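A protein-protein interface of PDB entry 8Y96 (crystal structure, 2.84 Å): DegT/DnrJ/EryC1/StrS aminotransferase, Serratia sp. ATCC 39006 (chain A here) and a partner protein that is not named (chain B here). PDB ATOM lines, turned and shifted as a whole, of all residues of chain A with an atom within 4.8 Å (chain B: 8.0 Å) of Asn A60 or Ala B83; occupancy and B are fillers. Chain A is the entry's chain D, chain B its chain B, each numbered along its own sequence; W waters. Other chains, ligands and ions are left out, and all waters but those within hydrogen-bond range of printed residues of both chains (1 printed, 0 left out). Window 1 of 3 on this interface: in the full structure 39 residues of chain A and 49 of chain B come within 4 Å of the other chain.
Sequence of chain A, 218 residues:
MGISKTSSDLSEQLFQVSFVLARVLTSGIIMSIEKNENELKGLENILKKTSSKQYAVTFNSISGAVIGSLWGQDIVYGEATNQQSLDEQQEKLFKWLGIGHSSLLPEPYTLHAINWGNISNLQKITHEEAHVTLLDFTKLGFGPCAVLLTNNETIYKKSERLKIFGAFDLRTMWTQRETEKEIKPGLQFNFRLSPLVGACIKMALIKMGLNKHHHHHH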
ATOM      1  N   THR A  58       2.665   4.908   1.423  1.00  0.00           N
ATOM      2  CA  THR A  58       3.677   5.891   1.784  1.00  0.00           C
ATOM      3  C   THR A  58       4.897   5.737   0.875  1.00  0.00           C
ATOM      4  O   THR A  58       5.208   4.640   0.417  1.00  0.00           O
ATOM      5  CB  THR A  58       4.064   5.754   3.253  1.00  0.00           C
ATOM      6  OG1 THR A  58       4.785   4.532   3.316  1.00  0.00           O
ATOM      7  CG2 THR A  58       2.864   5.729   4.182  1.00  0.00           C
ATOM      8  N   PHE A  59       5.585   6.861   0.646  1.00  0.00           N
ATOM      9  CA  PHE A  59       6.737   6.933  -0.237  1.00  0.00           C
ATOM     10  C   PHE A  59       7.836   7.758   0.432  1.00  0.00           C
ATOM     11  O   PHE A  59       7.554   8.565   1.314  1.00  0.00           O
ATOM     12  CB  PHE A  59       6.310   7.573  -1.562  1.00  0.00           C
ATOM     13  CG  PHE A  59       5.379   6.734  -2.427  1.00  0.00           C
ATOM     14  CD1 PHE A  59       5.887   5.770  -3.290  1.00  0.00           C
ATOM     15  CD2 PHE A  59       4.001   6.928  -2.394  1.00  0.00           C
ATOM     16  CE1 PHE A  59       5.043   5.012  -4.085  1.00  0.00           C
ATOM     17  CE2 PHE A  59       3.161   6.167  -3.194  1.00  0.00           C
ATOM     18  CZ  PHE A  59       3.682   5.211  -4.035  1.00  0.00           C
ATOM     19  N   ASN A  60       9.083   7.572  -0.019  1.00  0.00           N
ATOM     20  CA  ASN A  60      10.220   8.319   0.500  1.00  0.00           C
ATOM     21  C   ASN A  60      10.548   9.487  -0.426  1.00  0.00           C
ATOM     22  O   ASN A  60      11.622  10.079  -0.315  1.00  0.00           O
ATOM     23  CB  ASN A  60      11.438   7.423   0.698  1.00  0.00           C
ATOM     24  CG  ASN A  60      12.056   6.953  -0.600  1.00  0.00           C
ATOM     25  OD1 ASN A  60      11.862   7.564  -1.657  1.00  0.00           O
ATOM     26  ND2 ASN A  60      12.830   5.880  -0.537  1.00  0.00           N
ATOM     27  N   SER A  61       9.614   9.798  -1.334  1.00  0.00           N
ATOM     28  CA  SER A  61       9.815  10.803  -2.363  1.00  0.00           C
ATOM     29  C   SER A  61       8.479  11.138  -3.013  1.00  0.00           C
ATOM     30  O   SER A  61       7.645  10.258  -3.205  1.00  0.00           O
ATOM     31  CB  SER A  61      10.802  10.336  -3.395  1.00  0.00           C
ATOM     32  OG  SER A  61      10.821  11.226  -4.501  1.00  0.00           O
ATOM     33  N   ILE A  62       8.293  12.415  -3.361  1.00  0.00           N
ATOM     34  CA  ILE A  62       7.111  12.835  -4.097  1.00  0.00           C
ATOM     35  C   ILE A  62       7.070  12.069  -5.420  1.00  0.00           C
ATOM     36  O   ILE A  62       6.001  11.650  -5.862  1.00  0.00           O
ATOM     37  CB  ILE A  62       7.079  14.368  -4.280  1.00  0.00           C
ATOM     38  CG1 ILE A  62       5.765  14.843  -4.903  1.00  0.00           C
ATOM     39  CG2 ILE A  62       8.283  14.875  -5.077  1.00  0.00           C
ATOM     40  CD1 ILE A  62       4.526  14.464  -4.111  1.00  0.00           C
ATOM     41  N   PRO A 144      12.405  13.785   2.664  1.00  0.00           N
ATOM     42  CA  PRO A 144      11.410  13.659   1.598  1.00  0.00           C
ATOM     43  C   PRO A 144      10.426  12.533   1.902  1.00  0.00           C
ATOM     44  O   PRO A 144      10.838  11.434   2.263  1.00  0.00           O
ATOM     45  CB  PRO A 144      12.233  13.391   0.326  1.00  0.00           C
ATOM     46  CG  PRO A 144      13.650  13.782   0.696  1.00  0.00           C
ATOM     47  CD  PRO A 144      13.771  13.511   2.188  1.00  0.00           C
ATOM     48  N   CYS A 145       9.129  12.837   1.765  1.00  0.00           N
ATOM     49  CA  CYS A 145       8.069  11.885   2.055  1.00  0.00           C
ATOM     50  C   CYS A 145       6.776  12.314   1.368  1.00  0.00           C
ATOM     51  O   CYS A 145       6.459  13.500   1.315  1.00  0.00           O
ATOM     52  CB  CYS A 145       7.835  11.762   3.555  1.00  0.00           C
ATOM     53  SG  CYS A 145       6.398  10.741   3.966  1.00  0.00           S
ATOM     54  N   ASN A 190      13.217   1.847  -4.962  1.00  0.00           N
ATOM     55  CA  ASN A 190      13.141   1.846  -3.512  1.00  0.00           C
ATOM     56  C   ASN A 190      12.585   3.191  -3.068  1.00  0.00           C
ATOM     57  O   ASN A 190      13.338   4.142  -2.867  1.00  0.00           O
ATOM     58  CB  ASN A 190      14.484   1.548  -2.854  1.00  0.00           C
ATOM     59  CG  ASN A 190      14.374   1.454  -1.349  1.00  0.00           C
ATOM     60  OD1 ASN A 190      13.287   1.631  -0.785  1.00  0.00           O
ATOM     61  ND2 ASN A 190      15.479   1.161  -0.679  1.00  0.00           N
ATOM     62  N   PHE A 191      11.259   3.255  -2.947  1.00  0.00           N
ATOM     63  CA  PHE A 191      10.587   4.421  -2.398  1.00  0.00           C
ATOM     64  C   PHE A 191      10.055   4.088  -1.006  1.00  0.00           C
ATOM     65  O   PHE A 191       9.153   4.762  -0.512  1.00  0.00           O
ATOM     66  CB  PHE A 191       9.456   4.881  -3.321  1.00  0.00           C
ATOM     67  CG  PHE A 191       9.890   5.395  -4.688  1.00  0.00           C
ATOM     68  CD1 PHE A 191      10.983   6.244  -4.827  1.00  0.00           C
ATOM     69  CD2 PHE A 191       9.193   5.030  -5.831  1.00  0.00           C
ATOM     70  CE1 PHE A 191      11.361   6.717  -6.075  1.00  0.00           C
ATOM     71  CE2 PHE A 191       9.580   5.498  -7.078  1.00  0.00           C
ATOM     72  CZ  PHE A 191      10.666   6.337  -7.197  1.00  0.00           C
ATOM     73  N   ARG A 192      10.611   3.046  -0.377  1.00  0.00           N
ATOM     74  CA  ARG A 192      10.241   2.706   0.985  1.00  0.00           C
ATOM     75  C   ARG A 192      10.631   3.866   1.897  1.00  0.00           C
ATOM     76  O   ARG A 192      11.726   4.405   1.763  1.00  0.00           O
ATOM     77  CB  ARG A 192      10.942   1.422   1.445  1.00  0.00           C
ATOM     78  CG  ARG A 192      10.660   0.188   0.600  1.00  0.00           C
ATOM     79  CD  ARG A 192      11.108  -1.078   1.315  1.00  0.00           C
ATOM     80  NE  ARG A 192      12.557  -1.099   1.543  1.00  0.00           N
ATOM     81  CZ  ARG A 192      13.510  -1.401   0.664  1.00  0.00           C
ATOM     82  NH1 ARG A 192      13.223  -1.909  -0.524  1.00  0.00           N
ATOM     83  NH2 ARG A 192      14.776  -1.235   1.008  1.00  0.00           N
ATOM     84  N   LEU A 193       9.724   4.246   2.804  1.00  0.00           N
ATOM     85  CA  LEU A 193       9.964   5.339   3.734  1.00  0.00           C
ATOM     86  C   LEU A 193      10.577   4.786   5.015  1.00  0.00           C
ATOM     87  O   LEU A 193      10.257   3.679   5.437  1.00  0.00           O
ATOM     88  CB  LEU A 193       8.673   6.098   4.037  1.00  0.00           C
ATOM     89  CG  LEU A 193       8.815   7.332   4.936  1.00  0.00           C
ATOM     90  CD1 LEU A 193       9.558   8.447   4.219  1.00  0.00           C
ATOM     91  CD2 LEU A 193       7.462   7.819   5.420  1.00  0.00           C
ATOM     92  N   ILE B  80      27.363  11.419  -4.022  1.00  0.00           N
ATOM     93  CA  ILE B  80      26.013  11.949  -3.919  1.00  0.00           C
ATOM     94  C   ILE B  80      25.242  11.063  -2.940  1.00  0.00           C
ATOM     95  O   ILE B  80      25.188   9.849  -3.120  1.00  0.00           O
ATOM     96  CB  ILE B  80      25.326  12.013  -5.300  1.00  0.00           C
ATOM     97  CG1 ILE B  80      26.130  12.857  -6.302  1.00  0.00           C
ATOM     98  CG2 ILE B  80      23.887  12.518  -5.173  1.00  0.00           C
ATOM     99  CD1 ILE B  80      25.670  12.735  -7.746  1.00  0.00           C
ATOM    100  N   PRO B  81      24.649  11.631  -1.864  1.00  0.00           N
ATOM    101  CA  PRO B  81      23.812  10.854  -0.950  1.00  0.00           C
ATOM    102  C   PRO B  81      22.393  10.729  -1.494  1.00  0.00           C
ATOM    103  O   PRO B  81      21.830  11.709  -1.972  1.00  0.00           O
ATOM    104  CB  PRO B  81      23.890  11.697   0.333  1.00  0.00           C
ATOM    105  CG  PRO B  81      23.980  13.122  -0.167  1.00  0.00           C
ATOM    106  CD  PRO B  81      24.761  13.044  -1.468  1.00  0.00           C
ATOM    107  N   THR B  82      21.815   9.524  -1.419  1.00  0.00           N
ATOM    108  CA  THR B  82      20.500   9.283  -1.995  1.00  0.00           C
ATOM    109  C   THR B  82      19.541   8.783  -0.919  1.00  0.00           C
ATOM    110  O   THR B  82      19.909   8.649   0.246  1.00  0.00           O
ATOM    111  CB  THR B  82      20.590   8.282  -3.145  1.00  0.00           C
ATOM    112  OG1 THR B  82      20.854   7.024  -2.531  1.00  0.00           O
ATOM    113  CG2 THR B  82      21.658   8.649  -4.161  1.00  0.00           C
ATOM    114  N   ALA B  83      18.308   8.499  -1.358  1.00  0.00           N
ATOM    115  CA  ALA B  83      17.243   8.027  -0.490  1.00  0.00           C
ATOM    116  C   ALA B  83      17.284   6.509  -0.371  1.00  0.00           C
ATOM    117  O   ALA B  83      16.517   5.941   0.403  1.00  0.00           O
ATOM    118  CB  ALA B  83      15.910   8.477  -1.036  1.00  0.00           C
ATOM    119  N   SER B  84      18.166   5.864  -1.145  1.00  0.00           N
ATOM    120  CA  SER B  84      18.132   4.419  -1.286  1.00  0.00           C
ATOM    121  C   SER B  84      19.380   3.922  -2.001  1.00  0.00           C
ATOM    122  O   SER B  84      19.931   4.614  -2.856  1.00  0.00           O
ATOM    123  CB  SER B  84      16.903   3.987  -2.050  1.00  0.00           C
ATOM    124  OG  SER B  84      16.932   4.460  -3.392  1.00  0.00           O
ATOM    125  N   GLY B  85      19.774   2.686  -1.678  1.00  0.00           N
ATOM    126  CA  GLY B  85      20.781   1.974  -2.447  1.00  0.00           C
ATOM    127  C   GLY B  85      20.436   1.939  -3.935  1.00  0.00           C
ATOM    128  O   GLY B  85      21.314   2.128  -4.775  1.00  0.00           O
ATOM    129  N   THR B  86      19.153   1.714  -4.251  1.00  0.00           N
ATOM    130  CA  THR B  86      18.728   1.457  -5.621  1.00  0.00           C
ATOM    131  C   THR B  86      18.883   2.717  -6.470  1.00  0.00           C
ATOM    132  O   THR B  86      19.276   2.627  -7.631  1.00  0.00           O
ATOM    133  CB  THR B  86      17.288   0.949  -5.652  1.00  0.00           C
ATOM    134  OG1 THR B  86      17.215  -0.100  -4.692  1.00  0.00           O
ATOM    135  CG2 THR B  86      16.894   0.440  -7.026  1.00  0.00           C
ATOM    136  N   SER B  87      18.548   3.878  -5.891  1.00  0.00           N
ATOM    137  CA  SER B  87      18.659   5.150  -6.592  1.00  0.00           C
ATOM    138  C   SER B  87      20.124   5.493  -6.848  1.00  0.00           C
ATOM    139  O   SER B  87      20.454   6.071  -7.880  1.00  0.00           O
ATOM    140  CB  SER B  87      17.957   6.258  -5.839  1.00  0.00           C
ATOM    141  OG  SER B  87      18.345   6.287  -4.473  1.00  0.00           O
ATOM    142  N   SER B  88      20.999   5.124  -5.904  1.00  0.00           N
ATOM    143  CA  SER B  88      22.419   5.413  -6.015  1.00  0.00           C
ATOM    144  C   SER B  88      23.028   4.644  -7.185  1.00  0.00           C
ATOM    145  O   SER B  88      23.930   5.152  -7.846  1.00  0.00           O
ATOM    146  CB  SER B  88      23.148   5.128  -4.724  1.00  0.00           C
ATOM    147  OG  SER B  88      23.398   3.741  -4.546  1.00  0.00           O
ATOM    148  N   LEU B  91      21.976   6.352 -10.422  1.00  0.00           N
ATOM    149  CA  LEU B  91      22.811   7.523 -10.653  1.00  0.00           C
ATOM    150  C   LEU B  91      24.240   7.112 -11.012  1.00  0.00           C
ATOM    151  O   LEU B  91      24.888   7.760 -11.832  1.00  0.00           O
ATOM    152  CB  LEU B  91      22.790   8.411  -9.409  1.00  0.00           C
ATOM    153  CG  LEU B  91      21.426   8.977  -9.006  1.00  0.00           C
ATOM    154  CD1 LEU B  91      21.559   9.753  -7.712  1.00  0.00           C
ATOM    155  CD2 LEU B  91      20.822   9.853 -10.090  1.00  0.00           C
ATOM    156  N   LEU B 207      22.764   1.961   2.125  1.00  0.00           N
ATOM    157  CA  LEU B 207      23.088   2.308   3.499  1.00  0.00           C
ATOM    158  C   LEU B 207      21.854   2.064   4.362  1.00  0.00           C
ATOM    159  O   LEU B 207      21.586   2.806   5.306  1.00  0.00           O
ATOM    160  CB  LEU B 207      23.546   3.762   3.567  1.00  0.00           C
ATOM    161  CG  LEU B 207      24.806   4.110   2.772  1.00  0.00           C
ATOM    162  CD1 LEU B 207      25.022   5.612   2.756  1.00  0.00           C
ATOM    163  CD2 LEU B 207      26.011   3.390   3.350  1.00  0.00           C
ATOM    164  N   MET B 208      21.117   1.003   4.021  1.00  0.00           N
ATOM    165  CA  MET B 208      19.906   0.633   4.731  1.00  0.00           C
ATOM    166  C   MET B 208      20.301   0.028   6.079  1.00  0.00           C
ATOM    167  O   MET B 208      21.437  -0.411   6.251  1.00  0.00           O
ATOM    168  CB  MET B 208      19.095  -0.360   3.891  1.00  0.00           C
ATOM    169  CG  MET B 208      17.680  -0.585   4.371  1.00  0.00           C
ATOM    170  SD  MET B 208      16.929  -2.019   3.578  1.00  0.00           S
ATOM    171  CE  MET B 208      16.147  -2.680   5.057  1.00  0.00           C
ATOM    172  N   GLY B 217      17.362   3.851   8.548  1.00  0.00           N
ATOM    173  CA  GLY B 217      16.213   3.434   7.759  1.00  0.00           C
ATOM    174  C   GLY B 217      16.613   3.105   6.325  1.00  0.00           C
ATOM    175  O   GLY B 217      17.362   2.158   6.092  1.00  0.00           O
ATOM    176  N   GLU B 218      16.088   3.887   5.374  1.00  0.00           N
ATOM    177  CA  GLU B 218      16.444   3.757   3.972  1.00  0.00           C
ATOM    178  C   GLU B 218      17.460   4.846   3.645  1.00  0.00           C
ATOM    179  O   GLU B 218      17.318   5.983   4.094  1.00  0.00           O
ATOM    180  CB  GLU B 218      15.217   3.876   3.067  1.00  0.00           C
ATOM    181  CG  GLU B 218      14.107   2.878   3.395  1.00  0.00           C
ATOM    182  CD  GLU B 218      14.407   1.426   3.073  1.00  0.00           C
ATOM    183  OE1 GLU B 218      15.337   1.160   2.278  1.00  0.00           O
ATOM    184  OE2 GLU B 218      13.707   0.555   3.636  1.00  0.00           O
ATOM    185  N   ALA B 219      18.480   4.472   2.865  1.00  0.00           N
ATOM    186  CA  ALA B 219      19.552   5.379   2.486  1.00  0.00           C
ATOM    187  C   ALA B 219      20.496   4.675   1.522  1.00  0.00           C
ATOM    188  O   ALA B 219      20.625   3.455   1.552  1.00  0.00           O
ATOM    189  CB  ALA B 219      20.314   5.849   3.707  1.00  0.00           C
ATOM    190  N   GLY B 220      21.172   5.470   0.691  1.00  0.00           N
ATOM    191  CA  GLY B 220      22.233   4.960  -0.157  1.00  0.00           C
ATOM    192  C   GLY B 220      23.205   6.074  -0.517  1.00  0.00           C
ATOM    193  O   GLY B 220      22.960   7.233  -0.185  1.00  0.00           O
ATOM    194  N   ILE B 221      24.302   5.707  -1.191  1.00  0.00           N
ATOM    195  CA  ILE B 221      25.290   6.684  -1.614  1.00  0.00           C
ATOM    196  C   ILE B 221      25.942   6.207  -2.907  1.00  0.00           C
ATOM    197  O   ILE B 221      26.239   5.022  -3.060  1.00  0.00           O
ATOM    198  CB  ILE B 221      26.324   6.956  -0.502  1.00  0.00           C
ATOM    199  CG1 ILE B 221      27.189   8.172  -0.828  1.00  0.00           C
ATOM    200  CG2 ILE B 221      27.174   5.719  -0.214  1.00  0.00           C
ATOM    201  CD1 ILE B 221      27.919   8.749   0.369  1.00  0.00           C
ATOM    202  N   ASP B 243      13.275  13.094  -7.318  1.00  0.00           N
ATOM    203  CA  ASP B 243      13.711  13.499  -5.992  1.00  0.00           C
ATOM    204  C   ASP B 243      14.288  12.280  -5.272  1.00  0.00           C
ATOM    205  O   ASP B 243      13.546  11.499  -4.678  1.00  0.00           O
ATOM    206  CB  ASP B 243      12.578  14.152  -5.216  1.00  0.00           C
ATOM    207  CG  ASP B 243      12.934  14.678  -3.829  1.00  0.00           C
ATOM    208  OD1 ASP B 243      14.128  14.615  -3.461  1.00  0.00           O
ATOM    209  OD2 ASP B 243      12.009  15.148  -3.125  1.00  0.00           O
ATOM    210  N   TYR B 244      15.620  12.139  -5.330  1.00  0.00           N
ATOM    211  CA  TYR B 244      16.320  10.979  -4.794  1.00  0.00           C
ATOM    212  C   TYR B 244      17.083  11.363  -3.523  1.00  0.00           C
ATOM    213  O   TYR B 244      18.076  10.725  -3.178  1.00  0.00           O
ATOM    214  CB  TYR B 244      17.289  10.425  -5.851  1.00  0.00           C
ATOM    215  CG  TYR B 244      16.800   9.379  -6.850  1.00  0.00           C
ATOM    216  CD1 TYR B 244      15.632   8.644  -6.661  1.00  0.00           C
ATOM    217  CD2 TYR B 244      17.568   9.078  -7.970  1.00  0.00           C
ATOM    218  CE1 TYR B 244      15.227   7.681  -7.574  1.00  0.00           C
ATOM    219  CE2 TYR B 244      17.179   8.112  -8.885  1.00  0.00           C
ATOM    220  CZ  TYR B 244      16.005   7.412  -8.687  1.00  0.00           C
ATOM    221  OH  TYR B 244      15.633   6.457  -9.588  1.00  0.00           O
ATOM    222  N   ARG B 245      16.613  12.390  -2.808  1.00  0.00           N
ATOM    223  CA  ARG B 245      17.399  12.976  -1.734  1.00  0.00           C
ATOM    224  C   ARG B 245      17.280  12.148  -0.456  1.00  0.00           C
ATOM    225  O   ARG B 245      16.248  11.533  -0.194  1.00  0.00           O
ATOM    226  CB  ARG B 245      16.964  14.418  -1.463  1.00  0.00           C
ATOM    227  CG  ARG B 245      17.353  15.399  -2.559  1.00  0.00           C
ATOM    228  CD  ARG B 245      16.752  16.771  -2.294  1.00  0.00           C
ATOM    229  NE  ARG B 245      15.286  16.721  -2.278  1.00  0.00           N
ATOM    230  CZ  ARG B 245      14.480  17.682  -1.852  1.00  0.00           C
ATOM    231  NH1 ARG B 245      14.968  18.829  -1.423  1.00  0.00           N
ATOM    232  NH2 ARG B 245      13.173  17.494  -1.855  1.00  0.00           N
ATOM    233  N   MET B 246      18.356  12.179   0.344  1.00  0.00           N
ATOM    234  CA  MET B 246      18.423  11.480   1.617  1.00  0.00           C
ATOM    235  C   MET B 246      17.697  12.285   2.691  1.00  0.00           C
ATOM    236  O   MET B 246      17.600  13.507   2.601  1.00  0.00           O
ATOM    237  CB  MET B 246      19.881  11.277   2.047  1.00  0.00           C
ATOM    238  CG  MET B 246      20.061  10.513   3.352  1.00  0.00           C
ATOM    239  SD  MET B 246      21.792  10.231   3.771  1.00  0.00           S
ATOM    240  CE  MET B 246      22.340   9.175   2.421  1.00  0.00           C
ATOM    241  N   SER B 247      17.188  11.566   3.698  1.00  0.00           N
ATOM    242  CA  SER B 247      16.634  12.159   4.902  1.00  0.00           C
ATOM    243  C   SER B 247      17.764  12.477   5.874  1.00  0.00           C
ATOM    244  O   SER B 247      18.708  11.697   6.007  1.00  0.00           O
ATOM    245  CB  SER B 247      15.631  11.228   5.544  1.00  0.00           C
ATOM    246  OG  SER B 247      15.318  11.635   6.870  1.00  0.00           O
ATOM    247  N   ALA B 250      18.046   9.881   8.555  1.00  0.00           N
ATOM    248  CA  ALA B 250      18.761   8.690   8.132  1.00  0.00           C
ATOM    249  C   ALA B 250      20.264   8.926   8.242  1.00  0.00           C
ATOM    250  O   ALA B 250      20.995   8.046   8.691  1.00  0.00           O
ATOM    251  CB  ALA B 250      18.353   8.310   6.727  1.00  0.00           C
HETATM  252  O   HOH W   1      17.861   1.800   1.600  1.00  0.00           O
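The side-chain sulfur (SD) of Met B208 lies within hydrogen-bond range of the guanidinium group (NH2) of Arg A192 (3.4 Å).
The side-chain carboxylate (OE1) of Glu B218 is in hydrogen-bond range of the side-chain amide nitrogen (ND2) of Asn A190 (3.0 Å).
The guanidinium group of Arg A192 lies within salt-bridge range of the side-chain carboxylate of Glu B218 (2.8 Å).
The backbone carbonyl oxygen (O) of Asp B243 sits at hydrogen-bond distance from the side-chain hydroxyl (OG) of Ser A61 (2.7 Å).
Among the printed residues, merely in contact across the chains: Asn A60 with Ala B83 (3.8 Å), Pro A144 with Asp B243 (3.9 Å), Pro A144 with Arg B245 (3.5 Å), Pro A144 with Met B246 (3.9 Å), Asn A190 with Ser B84 (3.4 Å) and Asn A190 with Thr B86 (3.7 Å).
Water W1 lies within hydrogen-bond range of the side-chain carboxylate (OE1) of Glu B218 (2.7 Å), the backbone NH (N) of Ala B219 (3.0 Å) and the side-chain amide nitrogen (ND2) of Asn A190 (3.4 Å).
Of the 23 printed residues of chain B, 8 touch a printed residue of chain A.
Printed residues of chain B that touch a printed residue of chain A: Ala B83, Ser B84, Thr B86, Met B208, Glu B218, Asp B243, Arg B245 and Met B246.
Hydrophobic or aromatic side chains of chain B that line the printed part of chain A: Met B208.
Among the printed residues, 10 pairs touch across the chains.
Among the printed residues, Asp or Glu carboxylates within 4 Å of a Lys or Arg side-chain nitrogen of the other chain: Arg A192 with Glu B218 (2.8 Å).
Of chain B, only Ala B83 (3.8 Å) comes within 4 Å of Asn A60.
Printed residues of chain B within 4 Å of Ser A61: Asp B243.
Of the printed residues of chain B, Asn A190 touches Ser B84 (3.4 Å), Thr B86 (3.7 Å) and Glu B218 (3.0 Å).
Ala B83 touches just one residue of chain A: Asn A60.
Of the printed residues of chain A, Ser B84 touches Asn A190.
Printed residues of chain A within 4 Å of Glu B218: Asn A190 and Arg A192.
The nearest printed residue of chain B that does not touch Asn A60 is Ser B84 (4.7 Å).
The nearest printed residue of chain A that does not touch Ala B83 is Asn A190 (4.9 Å).
The nearest printed residue of chain B that does not touch Ser A61 is Tyr B244 (5.0 Å).
The backbone NH of Ala B83 sits at hydrogen-bond distance from the backbone carbonyl oxygen of Tyr B244 (2.9 Å).
The side-chain hydroxyl (OG) of Ser B84 sits at hydrogen-bond distance from the side-chain hydroxyl (OG) of Ser B87.
The side-chain amide nitrogen (ND2) of Asn A60 is in hydrogen-bond range of the backbone carbonyl oxygen (O) of Asn A190.
The backbone carbonyl oxygen (O) of Phe A191 sits at hydrogen-bond distance from the backbone NH (N) of Asn A60 (2.9 Å).
The side-chain amide nitrogen of Asn A60 lies within hydrogen-bond range of the backbone carbonyl oxygen of Arg A192, 2.9 Å away.
ND2 of Asn A190 sits close to NH2 of Arg A192 (3.0 Å).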
